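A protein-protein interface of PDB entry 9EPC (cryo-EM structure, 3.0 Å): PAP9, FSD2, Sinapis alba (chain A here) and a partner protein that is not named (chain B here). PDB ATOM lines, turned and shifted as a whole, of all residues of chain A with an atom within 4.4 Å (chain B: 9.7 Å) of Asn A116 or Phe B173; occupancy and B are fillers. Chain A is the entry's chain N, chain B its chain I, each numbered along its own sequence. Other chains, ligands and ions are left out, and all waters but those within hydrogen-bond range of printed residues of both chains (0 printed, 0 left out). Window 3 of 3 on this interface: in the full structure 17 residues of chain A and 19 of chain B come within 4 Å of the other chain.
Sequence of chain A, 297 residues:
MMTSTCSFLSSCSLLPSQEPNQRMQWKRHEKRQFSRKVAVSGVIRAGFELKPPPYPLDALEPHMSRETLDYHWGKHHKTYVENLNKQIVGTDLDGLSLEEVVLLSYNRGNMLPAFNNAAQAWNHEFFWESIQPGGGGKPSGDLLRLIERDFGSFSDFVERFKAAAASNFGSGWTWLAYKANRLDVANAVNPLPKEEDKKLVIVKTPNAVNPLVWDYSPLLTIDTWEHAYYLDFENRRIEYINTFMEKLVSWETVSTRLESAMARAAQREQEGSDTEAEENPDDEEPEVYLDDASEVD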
ATOM      1  N   PRO A 113     -25.645  31.123  26.392  1.00  0.00           N
ATOM      2  CA  PRO A 113     -25.561  29.921  25.545  1.00  0.00           C
ATOM      3  C   PRO A 113     -26.771  29.010  25.643  1.00  0.00           C
ATOM      4  O   PRO A 113     -27.119  28.351  24.655  1.00  0.00           O
ATOM      5  CB  PRO A 113     -24.289  29.226  26.050  1.00  0.00           C
ATOM      6  CG  PRO A 113     -24.096  29.749  27.435  1.00  0.00           C
ATOM      7  CD  PRO A 113     -24.558  31.171  27.382  1.00  0.00           C
ATOM      8  N   ALA A 114     -27.423  28.948  26.802  1.00  0.00           N
ATOM      9  CA  ALA A 114     -28.579  28.077  26.960  1.00  0.00           C
ATOM     10  C   ALA A 114     -29.829  28.615  26.279  1.00  0.00           C
ATOM     11  O   ALA A 114     -30.827  27.889  26.198  1.00  0.00           O
ATOM     12  CB  ALA A 114     -28.861  27.849  28.445  1.00  0.00           C
ATOM     13  N   PHE A 115     -29.803  29.857  25.793  1.00  0.00           N
ATOM     14  CA  PHE A 115     -31.008  30.454  25.225  1.00  0.00           C
ATOM     15  C   PHE A 115     -31.459  29.728  23.964  1.00  0.00           C
ATOM     16  O   PHE A 115     -32.657  29.489  23.775  1.00  0.00           O
ATOM     17  CB  PHE A 115     -30.772  31.934  24.929  1.00  0.00           C
ATOM     18  CG  PHE A 115     -31.905  32.590  24.197  1.00  0.00           C
ATOM     19  CD1 PHE A 115     -33.013  33.051  24.883  1.00  0.00           C
ATOM     20  CD2 PHE A 115     -31.861  32.745  22.823  1.00  0.00           C
ATOM     21  CE1 PHE A 115     -34.056  33.653  24.213  1.00  0.00           C
ATOM     22  CE2 PHE A 115     -32.902  33.345  22.148  1.00  0.00           C
ATOM     23  CZ  PHE A 115     -34.001  33.800  22.844  1.00  0.00           C
ATOM     24  N   ASN A 116     -30.518  29.378  23.084  1.00  0.00           N
ATOM     25  CA  ASN A 116     -30.889  28.823  21.786  1.00  0.00           C
ATOM     26  C   ASN A 116     -31.646  27.510  21.940  1.00  0.00           C
ATOM     27  O   ASN A 116     -32.680  27.297  21.297  1.00  0.00           O
ATOM     28  CB  ASN A 116     -29.644  28.630  20.923  1.00  0.00           C
ATOM     29  CG  ASN A 116     -29.043  29.941  20.471  1.00  0.00           C
ATOM     30  OD1 ASN A 116     -28.241  30.547  21.181  1.00  0.00           O
ATOM     31  ND2 ASN A 116     -29.430  30.390  19.284  1.00  0.00           N
ATOM     32  N   ASN A 117     -31.149  26.616  22.795  1.00  0.00           N
ATOM     33  CA  ASN A 117     -31.859  25.365  23.027  1.00  0.00           C
ATOM     34  C   ASN A 117     -33.174  25.608  23.752  1.00  0.00           C
ATOM     35  O   ASN A 117     -34.168  24.919  23.496  1.00  0.00           O
ATOM     36  CB  ASN A 117     -30.979  24.396  23.816  1.00  0.00           C
ATOM     37  CG  ASN A 117     -29.768  23.942  23.031  1.00  0.00           C
ATOM     38  OD1 ASN A 117     -29.828  22.965  22.287  1.00  0.00           O
ATOM     39  ND2 ASN A 117     -28.658  24.651  23.194  1.00  0.00           N
ATOM     40  N   ALA A 118     -33.199  26.584  24.662  1.00  0.00           N
ATOM     41  CA  ALA A 118     -34.422  26.875  25.399  1.00  0.00           C
ATOM     42  C   ALA A 118     -35.516  27.383  24.470  1.00  0.00           C
ATOM     43  O   ALA A 118     -36.663  26.924  24.532  1.00  0.00           O
ATOM     44  CB  ALA A 118     -34.136  27.893  26.503  1.00  0.00           C
ATOM     45  N   ALA A 119     -35.177  28.332  23.596  1.00  0.00           N
ATOM     46  CA  ALA A 119     -36.172  28.870  22.675  1.00  0.00           C
ATOM     47  C   ALA A 119     -36.661  27.801  21.709  1.00  0.00           C
ATOM     48  O   ALA A 119     -37.865  27.693  21.450  1.00  0.00           O
ATOM     49  CB  ALA A 119     -35.592  30.059  21.913  1.00  0.00           C
ATOM     50  N   GLN A 120     -35.744  26.995  21.174  1.00  0.00           N
ATOM     51  CA  GLN A 120     -36.139  25.937  20.251  1.00  0.00           C
ATOM     52  C   GLN A 120     -37.039  24.918  20.934  1.00  0.00           C
ATOM     53  O   GLN A 120     -37.991  24.414  20.325  1.00  0.00           O
ATOM     54  CB  GLN A 120     -34.905  25.255  19.670  1.00  0.00           C
ATOM     55  CG  GLN A 120     -34.230  26.034  18.561  1.00  0.00           C
ATOM     56  CD  GLN A 120     -35.110  26.186  17.336  1.00  0.00           C
ATOM     57  OE1 GLN A 120     -35.940  27.092  17.261  1.00  0.00           O
ATOM     58  NE2 GLN A 120     -34.931  25.296  16.368  1.00  0.00           N
ATOM     59  N   ASN A 207     -33.759  32.334  13.126  1.00  0.00           N
ATOM     60  CA  ASN A 207     -33.190  31.285  13.967  1.00  0.00           C
ATOM     61  C   ASN A 207     -34.150  30.813  15.050  1.00  0.00           C
ATOM     62  O   ASN A 207     -35.151  30.153  14.758  1.00  0.00           O
ATOM     63  CB  ASN A 207     -31.887  31.768  14.604  1.00  0.00           C
ATOM     64  CG  ASN A 207     -30.760  31.882  13.605  1.00  0.00           C
ATOM     65  OD1 ASN A 207     -30.635  32.885  12.906  1.00  0.00           O
ATOM     66  ND2 ASN A 207     -29.928  30.851  13.530  1.00  0.00           N
ATOM     67  N   ALA A 208     -33.852  31.149  16.306  1.00  0.00           N
ATOM     68  CA  ALA A 208     -34.651  30.722  17.454  1.00  0.00           C
ATOM     69  C   ALA A 208     -34.886  31.927  18.360  1.00  0.00           C
ATOM     70  O   ALA A 208     -34.096  32.205  19.264  1.00  0.00           O
ATOM     71  CB  ALA A 208     -33.967  29.585  18.197  1.00  0.00           C
ATOM     72  N   TRP A 225     -37.983  26.702   9.552  1.00  0.00           N
ATOM     73  CA  TRP A 225     -36.694  26.035   9.450  1.00  0.00           C
ATOM     74  C   TRP A 225     -36.759  24.946   8.389  1.00  0.00           C
ATOM     75  O   TRP A 225     -37.753  24.225   8.280  1.00  0.00           O
ATOM     76  CB  TRP A 225     -36.301  25.429  10.794  1.00  0.00           C
ATOM     77  CG  TRP A 225     -35.719  26.400  11.761  1.00  0.00           C
ATOM     78  CD1 TRP A 225     -36.321  27.509  12.272  1.00  0.00           C
ATOM     79  CD2 TRP A 225     -34.420  26.338  12.356  1.00  0.00           C
ATOM     80  NE1 TRP A 225     -35.473  28.150  13.141  1.00  0.00           N
ATOM     81  CE2 TRP A 225     -34.298  27.449  13.212  1.00  0.00           C
ATOM     82  CE3 TRP A 225     -33.345  25.452  12.246  1.00  0.00           C
ATOM     83  CZ2 TRP A 225     -33.146  27.698  13.951  1.00  0.00           C
ATOM     84  CZ3 TRP A 225     -32.203  25.701  12.980  1.00  0.00           C
ATOM     85  CH2 TRP A 225     -32.113  26.813  13.822  1.00  0.00           C
ATOM     86  N   ASN B 167     -15.495  22.960  14.698  1.00  0.00           N
ATOM     87  CA  ASN B 167     -16.182  23.578  15.827  1.00  0.00           C
ATOM     88  C   ASN B 167     -16.977  24.796  15.382  1.00  0.00           C
ATOM     89  O   ASN B 167     -18.109  25.007  15.835  1.00  0.00           O
ATOM     90  CB  ASN B 167     -15.179  23.961  16.914  1.00  0.00           C
ATOM     91  CG  ASN B 167     -14.597  22.755  17.617  1.00  0.00           C
ATOM     92  OD1 ASN B 167     -15.258  21.727  17.760  1.00  0.00           O
ATOM     93  ND2 ASN B 167     -13.351  22.873  18.059  1.00  0.00           N
ATOM     94  N   ALA B 168     -16.403  25.609  14.495  1.00  0.00           N
ATOM     95  CA  ALA B 168     -17.145  26.739  13.949  1.00  0.00           C
ATOM     96  C   ALA B 168     -18.356  26.265  13.160  1.00  0.00           C
ATOM     97  O   ALA B 168     -19.439  26.854  13.251  1.00  0.00           O
ATOM     98  CB  ALA B 168     -16.230  27.594  13.073  1.00  0.00           C
ATOM     99  N   ALA B 169     -18.193  25.196  12.379  1.00  0.00           N
ATOM    100  CA  ALA B 169     -19.314  24.661  11.615  1.00  0.00           C
ATOM    101  C   ALA B 169     -20.386  24.082  12.529  1.00  0.00           C
ATOM    102  O   ALA B 169     -21.584  24.272  12.287  1.00  0.00           O
ATOM    103  CB  ALA B 169     -18.815  23.606  10.630  1.00  0.00           C
ATOM    104  N   LEU B 170     -19.979  23.371  13.582  1.00  0.00           N
ATOM    105  CA  LEU B 170     -20.952  22.782  14.496  1.00  0.00           C
ATOM    106  C   LEU B 170     -21.679  23.853  15.298  1.00  0.00           C
ATOM    107  O   LEU B 170     -22.908  23.814  15.435  1.00  0.00           O
ATOM    108  CB  LEU B 170     -20.261  21.789  15.430  1.00  0.00           C
ATOM    109  CG  LEU B 170     -19.801  20.478  14.794  1.00  0.00           C
ATOM    110  CD1 LEU B 170     -19.042  19.632  15.802  1.00  0.00           C
ATOM    111  CD2 LEU B 170     -20.991  19.713  14.239  1.00  0.00           C
ATOM    112  N   THR B 171     -20.939  24.825  15.833  1.00  0.00           N
ATOM    113  CA  THR B 171     -21.551  25.860  16.655  1.00  0.00           C
ATOM    114  C   THR B 171     -22.395  26.836  15.849  1.00  0.00           C
ATOM    115  O   THR B 171     -23.131  27.628  16.448  1.00  0.00           O
ATOM    116  CB  THR B 171     -20.479  26.631  17.426  1.00  0.00           C
ATOM    117  OG1 THR B 171     -19.451  27.057  16.524  1.00  0.00           O
ATOM    118  CG2 THR B 171     -19.869  25.753  18.509  1.00  0.00           C
ATOM    119  N   GLN B 172     -22.309  26.807  14.522  1.00  0.00           N
ATOM    120  CA  GLN B 172     -23.125  27.682  13.690  1.00  0.00           C
ATOM    121  C   GLN B 172     -24.586  27.279  13.821  1.00  0.00           C
ATOM    122  O   GLN B 172     -24.999  26.232  13.314  1.00  0.00           O
ATOM    123  CB  GLN B 172     -22.667  27.615  12.237  1.00  0.00           C
ATOM    124  CG  GLN B 172     -23.563  28.375  11.274  1.00  0.00           C
ATOM    125  CD  GLN B 172     -23.659  29.851  11.606  1.00  0.00           C
ATOM    126  OE1 GLN B 172     -22.710  30.450  12.111  1.00  0.00           O
ATOM    127  NE2 GLN B 172     -24.813  30.445  11.326  1.00  0.00           N
ATOM    128  N   PHE B 173     -25.369  28.106  14.504  1.00  0.00           N
ATOM    129  CA  PHE B 173     -26.771  27.811  14.754  1.00  0.00           C
ATOM    130  C   PHE B 173     -27.621  28.348  13.612  1.00  0.00           C
ATOM    131  O   PHE B 173     -27.503  29.519  13.238  1.00  0.00           O
ATOM    132  CB  PHE B 173     -27.218  28.417  16.083  1.00  0.00           C
ATOM    133  CG  PHE B 173     -28.624  28.068  16.461  1.00  0.00           C
ATOM    134  CD1 PHE B 173     -28.914  26.844  17.035  1.00  0.00           C
ATOM    135  CD2 PHE B 173     -29.655  28.964  16.248  1.00  0.00           C
ATOM    136  CE1 PHE B 173     -30.207  26.519  17.385  1.00  0.00           C
ATOM    137  CE2 PHE B 173     -30.949  28.645  16.595  1.00  0.00           C
ATOM    138  CZ  PHE B 173     -31.226  27.421  17.165  1.00  0.00           C
ATOM    139  N   GLY B 174     -28.473  27.492  13.063  1.00  0.00           N
ATOM    140  CA  GLY B 174     -29.318  27.884  11.960  1.00  0.00           C
ATOM    141  C   GLY B 174     -28.564  27.939  10.646  1.00  0.00           C
ATOM    142  O   GLY B 174     -27.424  27.487  10.517  1.00  0.00           O
ATOM    143  N   SER B 175     -29.235  28.508   9.650  1.00  0.00           N
ATOM    144  CA  SER B 175     -28.646  28.632   8.325  1.00  0.00           C
ATOM    145  C   SER B 175     -27.442  29.565   8.360  1.00  0.00           C
ATOM    146  O   SER B 175     -27.444  30.584   9.055  1.00  0.00           O
ATOM    147  CB  SER B 175     -29.682  29.152   7.331  1.00  0.00           C
ATOM    148  OG  SER B 175     -30.814  28.301   7.286  1.00  0.00           O
ATOM    149  N   GLY B 176     -26.412  29.212   7.602  1.00  0.00           N
ATOM    150  CA  GLY B 176     -25.215  30.027   7.568  1.00  0.00           C
ATOM    151  C   GLY B 176     -24.158  29.395   6.692  1.00  0.00           C
ATOM    152  O   GLY B 176     -24.406  28.411   5.994  1.00  0.00           O
ATOM    153  N   TRP B 177     -22.966  29.983   6.735  1.00  0.00           N
ATOM    154  CA  TRP B 177     -21.837  29.489   5.964  1.00  0.00           C
ATOM    155  C   TRP B 177     -20.599  29.462   6.843  1.00  0.00           C
ATOM    156  O   TRP B 177     -20.478  30.234   7.798  1.00  0.00           O
ATOM    157  CB  TRP B 177     -21.573  30.353   4.726  1.00  0.00           C
ATOM    158  CG  TRP B 177     -22.679  30.342   3.728  1.00  0.00           C
ATOM    159  CD1 TRP B 177     -23.872  30.989   3.824  1.00  0.00           C
ATOM    160  CD2 TRP B 177     -22.691  29.658   2.473  1.00  0.00           C
ATOM    161  NE1 TRP B 177     -24.632  30.747   2.709  1.00  0.00           N
ATOM    162  CE2 TRP B 177     -23.928  29.932   1.862  1.00  0.00           C
ATOM    163  CE3 TRP B 177     -21.777  28.839   1.806  1.00  0.00           C
ATOM    164  CZ2 TRP B 177     -24.276  29.415   0.618  1.00  0.00           C
ATOM    165  CZ3 TRP B 177     -22.123  28.330   0.572  1.00  0.00           C
ATOM    166  CH2 TRP B 177     -23.361  28.619  -0.010  1.00  0.00           C
ATOM    167  N   VAL B 178     -19.679  28.562   6.509  1.00  0.00           N
ATOM    168  CA  VAL B 178     -18.391  28.455   7.182  1.00  0.00           C
ATOM    169  C   VAL B 178     -17.324  28.902   6.196  1.00  0.00           C
ATOM    170  O   VAL B 178     -17.231  28.364   5.086  1.00  0.00           O
ATOM    171  CB  VAL B 178     -18.123  27.028   7.678  1.00  0.00           C
ATOM    172  CG1 VAL B 178     -16.830  26.982   8.473  1.00  0.00           C
ATOM    173  CG2 VAL B 178     -19.285  26.549   8.518  1.00  0.00           C
ATOM    174  N   LYS B 193     -17.582  32.190  11.101  1.00  0.00           N
ATOM    175  CA  LYS B 193     -18.934  31.698  10.885  1.00  0.00           C
ATOM    176  C   LYS B 193     -19.857  32.879  10.623  1.00  0.00           C
ATOM    177  O   LYS B 193     -19.856  33.855  11.381  1.00  0.00           O
ATOM    178  CB  LYS B 193     -19.428  30.894  12.089  1.00  0.00           C
ATOM    179  CG  LYS B 193     -19.250  31.599  13.426  1.00  0.00           C
ATOM    180  CD  LYS B 193     -20.259  31.112  14.450  1.00  0.00           C
ATOM    181  CE  LYS B 193     -20.107  29.628  14.714  1.00  0.00           C
ATOM    182  NZ  LYS B 193     -18.787  29.307  15.321  1.00  0.00           N
ATOM    183  N   THR B 194     -20.626  32.800   9.541  1.00  0.00           N
ATOM    184  CA  THR B 194     -21.573  33.847   9.183  1.00  0.00           C
ATOM    185  C   THR B 194     -22.932  33.217   8.932  1.00  0.00           C
ATOM    186  O   THR B 194     -23.039  32.245   8.178  1.00  0.00           O
ATOM    187  CB  THR B 194     -21.115  34.623   7.946  1.00  0.00           C
ATOM    188  OG1 THR B 194     -21.022  33.733   6.828  1.00  0.00           O
ATOM    189  CG2 THR B 194     -19.761  35.267   8.187  1.00  0.00           C
ATOM    190  N   SER B 195     -23.962  33.771   9.562  1.00  0.00           N
ATOM    191  CA  SER B 195     -25.306  33.230   9.443  1.00  0.00           C
ATOM    192  C   SER B 195     -26.005  33.773   8.204  1.00  0.00           C
ATOM    193  O   SER B 195     -25.733  34.888   7.748  1.00  0.00           O
ATOM    194  CB  SER B 195     -26.126  33.564  10.688  1.00  0.00           C
ATOM    195  OG  SER B 195     -26.176  34.963  10.898  1.00  0.00           O
ATOM    196  N   ASN B 196     -26.913  32.965   7.662  1.00  0.00           N
ATOM    197  CA  ASN B 196     -27.733  33.316   6.495  1.00  0.00           C
ATOM    198  C   ASN B 196     -26.792  33.608   5.329  1.00  0.00           C
ATOM    199  O   ASN B 196     -25.849  32.833   5.103  1.00  0.00           O
ATOM    200  CB  ASN B 196     -28.689  34.438   6.871  1.00  0.00           C
ATOM    201  CG  ASN B 196     -29.753  33.987   7.846  1.00  0.00           C
ATOM    202  OD1 ASN B 196     -30.079  32.802   7.920  1.00  0.00           O
ATOM    203  ND2 ASN B 196     -30.306  34.929   8.597  1.00  0.00           N
ATOM    204  N   VAL B 213     -23.560  25.221   5.473  1.00  0.00           N
ATOM    205  CA  VAL B 213     -24.242  24.502   6.540  1.00  0.00           C
ATOM    206  C   VAL B 213     -25.740  24.773   6.538  1.00  0.00           C
ATOM    207  O   VAL B 213     -26.425  24.460   7.517  1.00  0.00           O
ATOM    208  CB  VAL B 213     -23.629  24.821   7.912  1.00  0.00           C
ATOM    209  CG1 VAL B 213     -22.167  24.419   7.939  1.00  0.00           C
ATOM    210  CG2 VAL B 213     -23.789  26.290   8.240  1.00  0.00           C
ATOM    211  N   TRP B 214     -26.267  25.360   5.465  1.00  0.00           N
ATOM    212  CA  TRP B 214     -27.709  25.448   5.304  1.00  0.00           C
ATOM    213  C   TRP B 214     -28.310  24.051   5.281  1.00  0.00           C
ATOM    214  O   TRP B 214     -27.746  23.124   4.692  1.00  0.00           O
ATOM    215  CB  TRP B 214     -28.061  26.191   4.017  1.00  0.00           C
ATOM    216  CG  TRP B 214     -27.985  27.679   4.125  1.00  0.00           C
ATOM    217  CD1 TRP B 214     -26.890  28.421   4.439  1.00  0.00           C
ATOM    218  CD2 TRP B 214     -29.048  28.610   3.899  1.00  0.00           C
ATOM    219  NE1 TRP B 214     -27.204  29.756   4.436  1.00  0.00           N
ATOM    220  CE2 TRP B 214     -28.524  29.900   4.104  1.00  0.00           C
ATOM    221  CE3 TRP B 214     -30.394  28.478   3.547  1.00  0.00           C
ATOM    222  CZ2 TRP B 214     -29.297  31.048   3.971  1.00  0.00           C
ATOM    223  CZ3 TRP B 214     -31.159  29.618   3.414  1.00  0.00           C
ATOM    224  CH2 TRP B 214     -30.609  30.887   3.623  1.00  0.00           C
ATOM    225  N   GLU B 215     -29.466  23.901   5.928  1.00  0.00           N
ATOM    226  CA  GLU B 215     -30.071  22.580   6.055  1.00  0.00           C
ATOM    227  C   GLU B 215     -30.421  21.984   4.698  1.00  0.00           C
ATOM    228  O   GLU B 215     -30.478  20.757   4.559  1.00  0.00           O
ATOM    229  CB  GLU B 215     -31.311  22.655   6.943  1.00  0.00           C
ATOM    230  CG  GLU B 215     -31.011  23.059   8.375  1.00  0.00           C
ATOM    231  CD  GLU B 215     -32.257  23.152   9.231  1.00  0.00           C
ATOM    232  OE1 GLU B 215     -33.364  23.255   8.664  1.00  0.00           O
ATOM    233  OE2 GLU B 215     -32.129  23.121  10.473  1.00  0.00           O
ATOM    234  N   TYR B 218     -27.597  19.445   3.168  1.00  0.00           N
ATOM    235  CA  TYR B 218     -27.230  18.140   3.702  1.00  0.00           C
ATOM    236  C   TYR B 218     -28.395  17.294   4.189  1.00  0.00           C
ATOM    237  O   TYR B 218     -28.179  16.113   4.475  1.00  0.00           O
ATOM    238  CB  TYR B 218     -26.232  18.305   4.858  1.00  0.00           C
ATOM    239  CG  TYR B 218     -26.745  19.152   6.001  1.00  0.00           C
ATOM    240  CD1 TYR B 218     -27.465  18.585   7.044  1.00  0.00           C
ATOM    241  CD2 TYR B 218     -26.502  20.517   6.041  1.00  0.00           C
ATOM    242  CE1 TYR B 218     -27.933  19.355   8.090  1.00  0.00           C
ATOM    243  CE2 TYR B 218     -26.965  21.294   7.084  1.00  0.00           C
ATOM    244  CZ  TYR B 218     -27.680  20.708   8.105  1.00  0.00           C
ATOM    245  OH  TYR B 218     -28.145  21.478   9.146  1.00  0.00           O
ATOM    246  N   ARG B 226     -25.150  16.448  10.938  1.00  0.00           N
ATOM    247  CA  ARG B 226     -24.337  17.505  10.347  1.00  0.00           C
ATOM    248  C   ARG B 226     -22.852  17.208  10.506  1.00  0.00           C
ATOM    249  O   ARG B 226     -22.062  17.444   9.585  1.00  0.00           O
ATOM    250  CB  ARG B 226     -24.681  18.857  10.976  1.00  0.00           C
ATOM    251  CG  ARG B 226     -23.942  20.020  10.334  1.00  0.00           C
ATOM    252  CD  ARG B 226     -24.026  21.291  11.164  1.00  0.00           C
ATOM    253  NE  ARG B 226     -25.327  21.942  11.060  1.00  0.00           N
ATOM    254  CZ  ARG B 226     -25.596  23.151  11.532  1.00  0.00           C
ATOM    255  NH1 ARG B 226     -24.674  23.874  12.146  1.00  0.00           N
ATOM    256  NH2 ARG B 226     -26.820  23.649  11.382  1.00  0.00           N
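ND2 of Asn A207 is in hydrogen-bond range of O of Phe B173 (2.8 Å).
The backbone carbonyl oxygen (O) of Asn A207 sits at hydrogen-bond distance from the indole nitrogen (NE1) of Trp A225 (2.6 Å).
Asn A116 touches Phe B173 (ND2 to CD2, 3.4 Å). CG of Gln A120 touches CZ of Phe B173, at 3.6 Å. Asn A207 touches Gly B174 (ND2 to CA, 3.4 Å). CE2 of Phe B173 touches CB of Ala A208, 3.5 Å away. Trp A225 touches Phe B173. Trp A225 touches Gly B174. Trp A225 touches Glu B215 (CE3 to OE2, 3.2 Å).
Of the printed residues of chain B, Asn A116 touches Phe B173 (3.4 Å). No residue of chain B comes within 4 Å of Asn A117. Ala A118 touches none of the printed residues of chain B. No residue of chain B comes within 4 Å of Ala A119. Of the printed residues of chain B, Gln A120 touches Phe B173 (3.6 Å). Ala A208 touches just one residue of chain B: Phe B173 (3.5 Å). Of the printed residues of chain B, Trp A225 touches Phe B173 (3.5 Å), Gly B174 (3.5 Å) and Glu B215 (3.2 Å). Of the printed residues of chain A, Phe B173 touches Asn A116 (3.4 Å), Gln A120 (3.6 Å), Asn A207 (2.8 Å), Ala A208 (3.5 Å) and Trp A225 (3.5 Å). Printed residues of chain A within 4 Å of Gly B174: Asn A207 and Trp A225. The nearest residue of chain B that does not touch Asn A116 is Gly B174 (6.9 Å).
Printed residues of chain A that touch a printed residue of chain B: Asn A116, Gln A120, Asn A207, Ala A208 and Trp A225. Hydrophobic or aromatic side chains of chain A within 4 Å of the printed part of chain B: Ala A208 and Trp A225. Hydrophobic or aromatic side chains of chain B that line the printed part of chain A: Phe B173.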
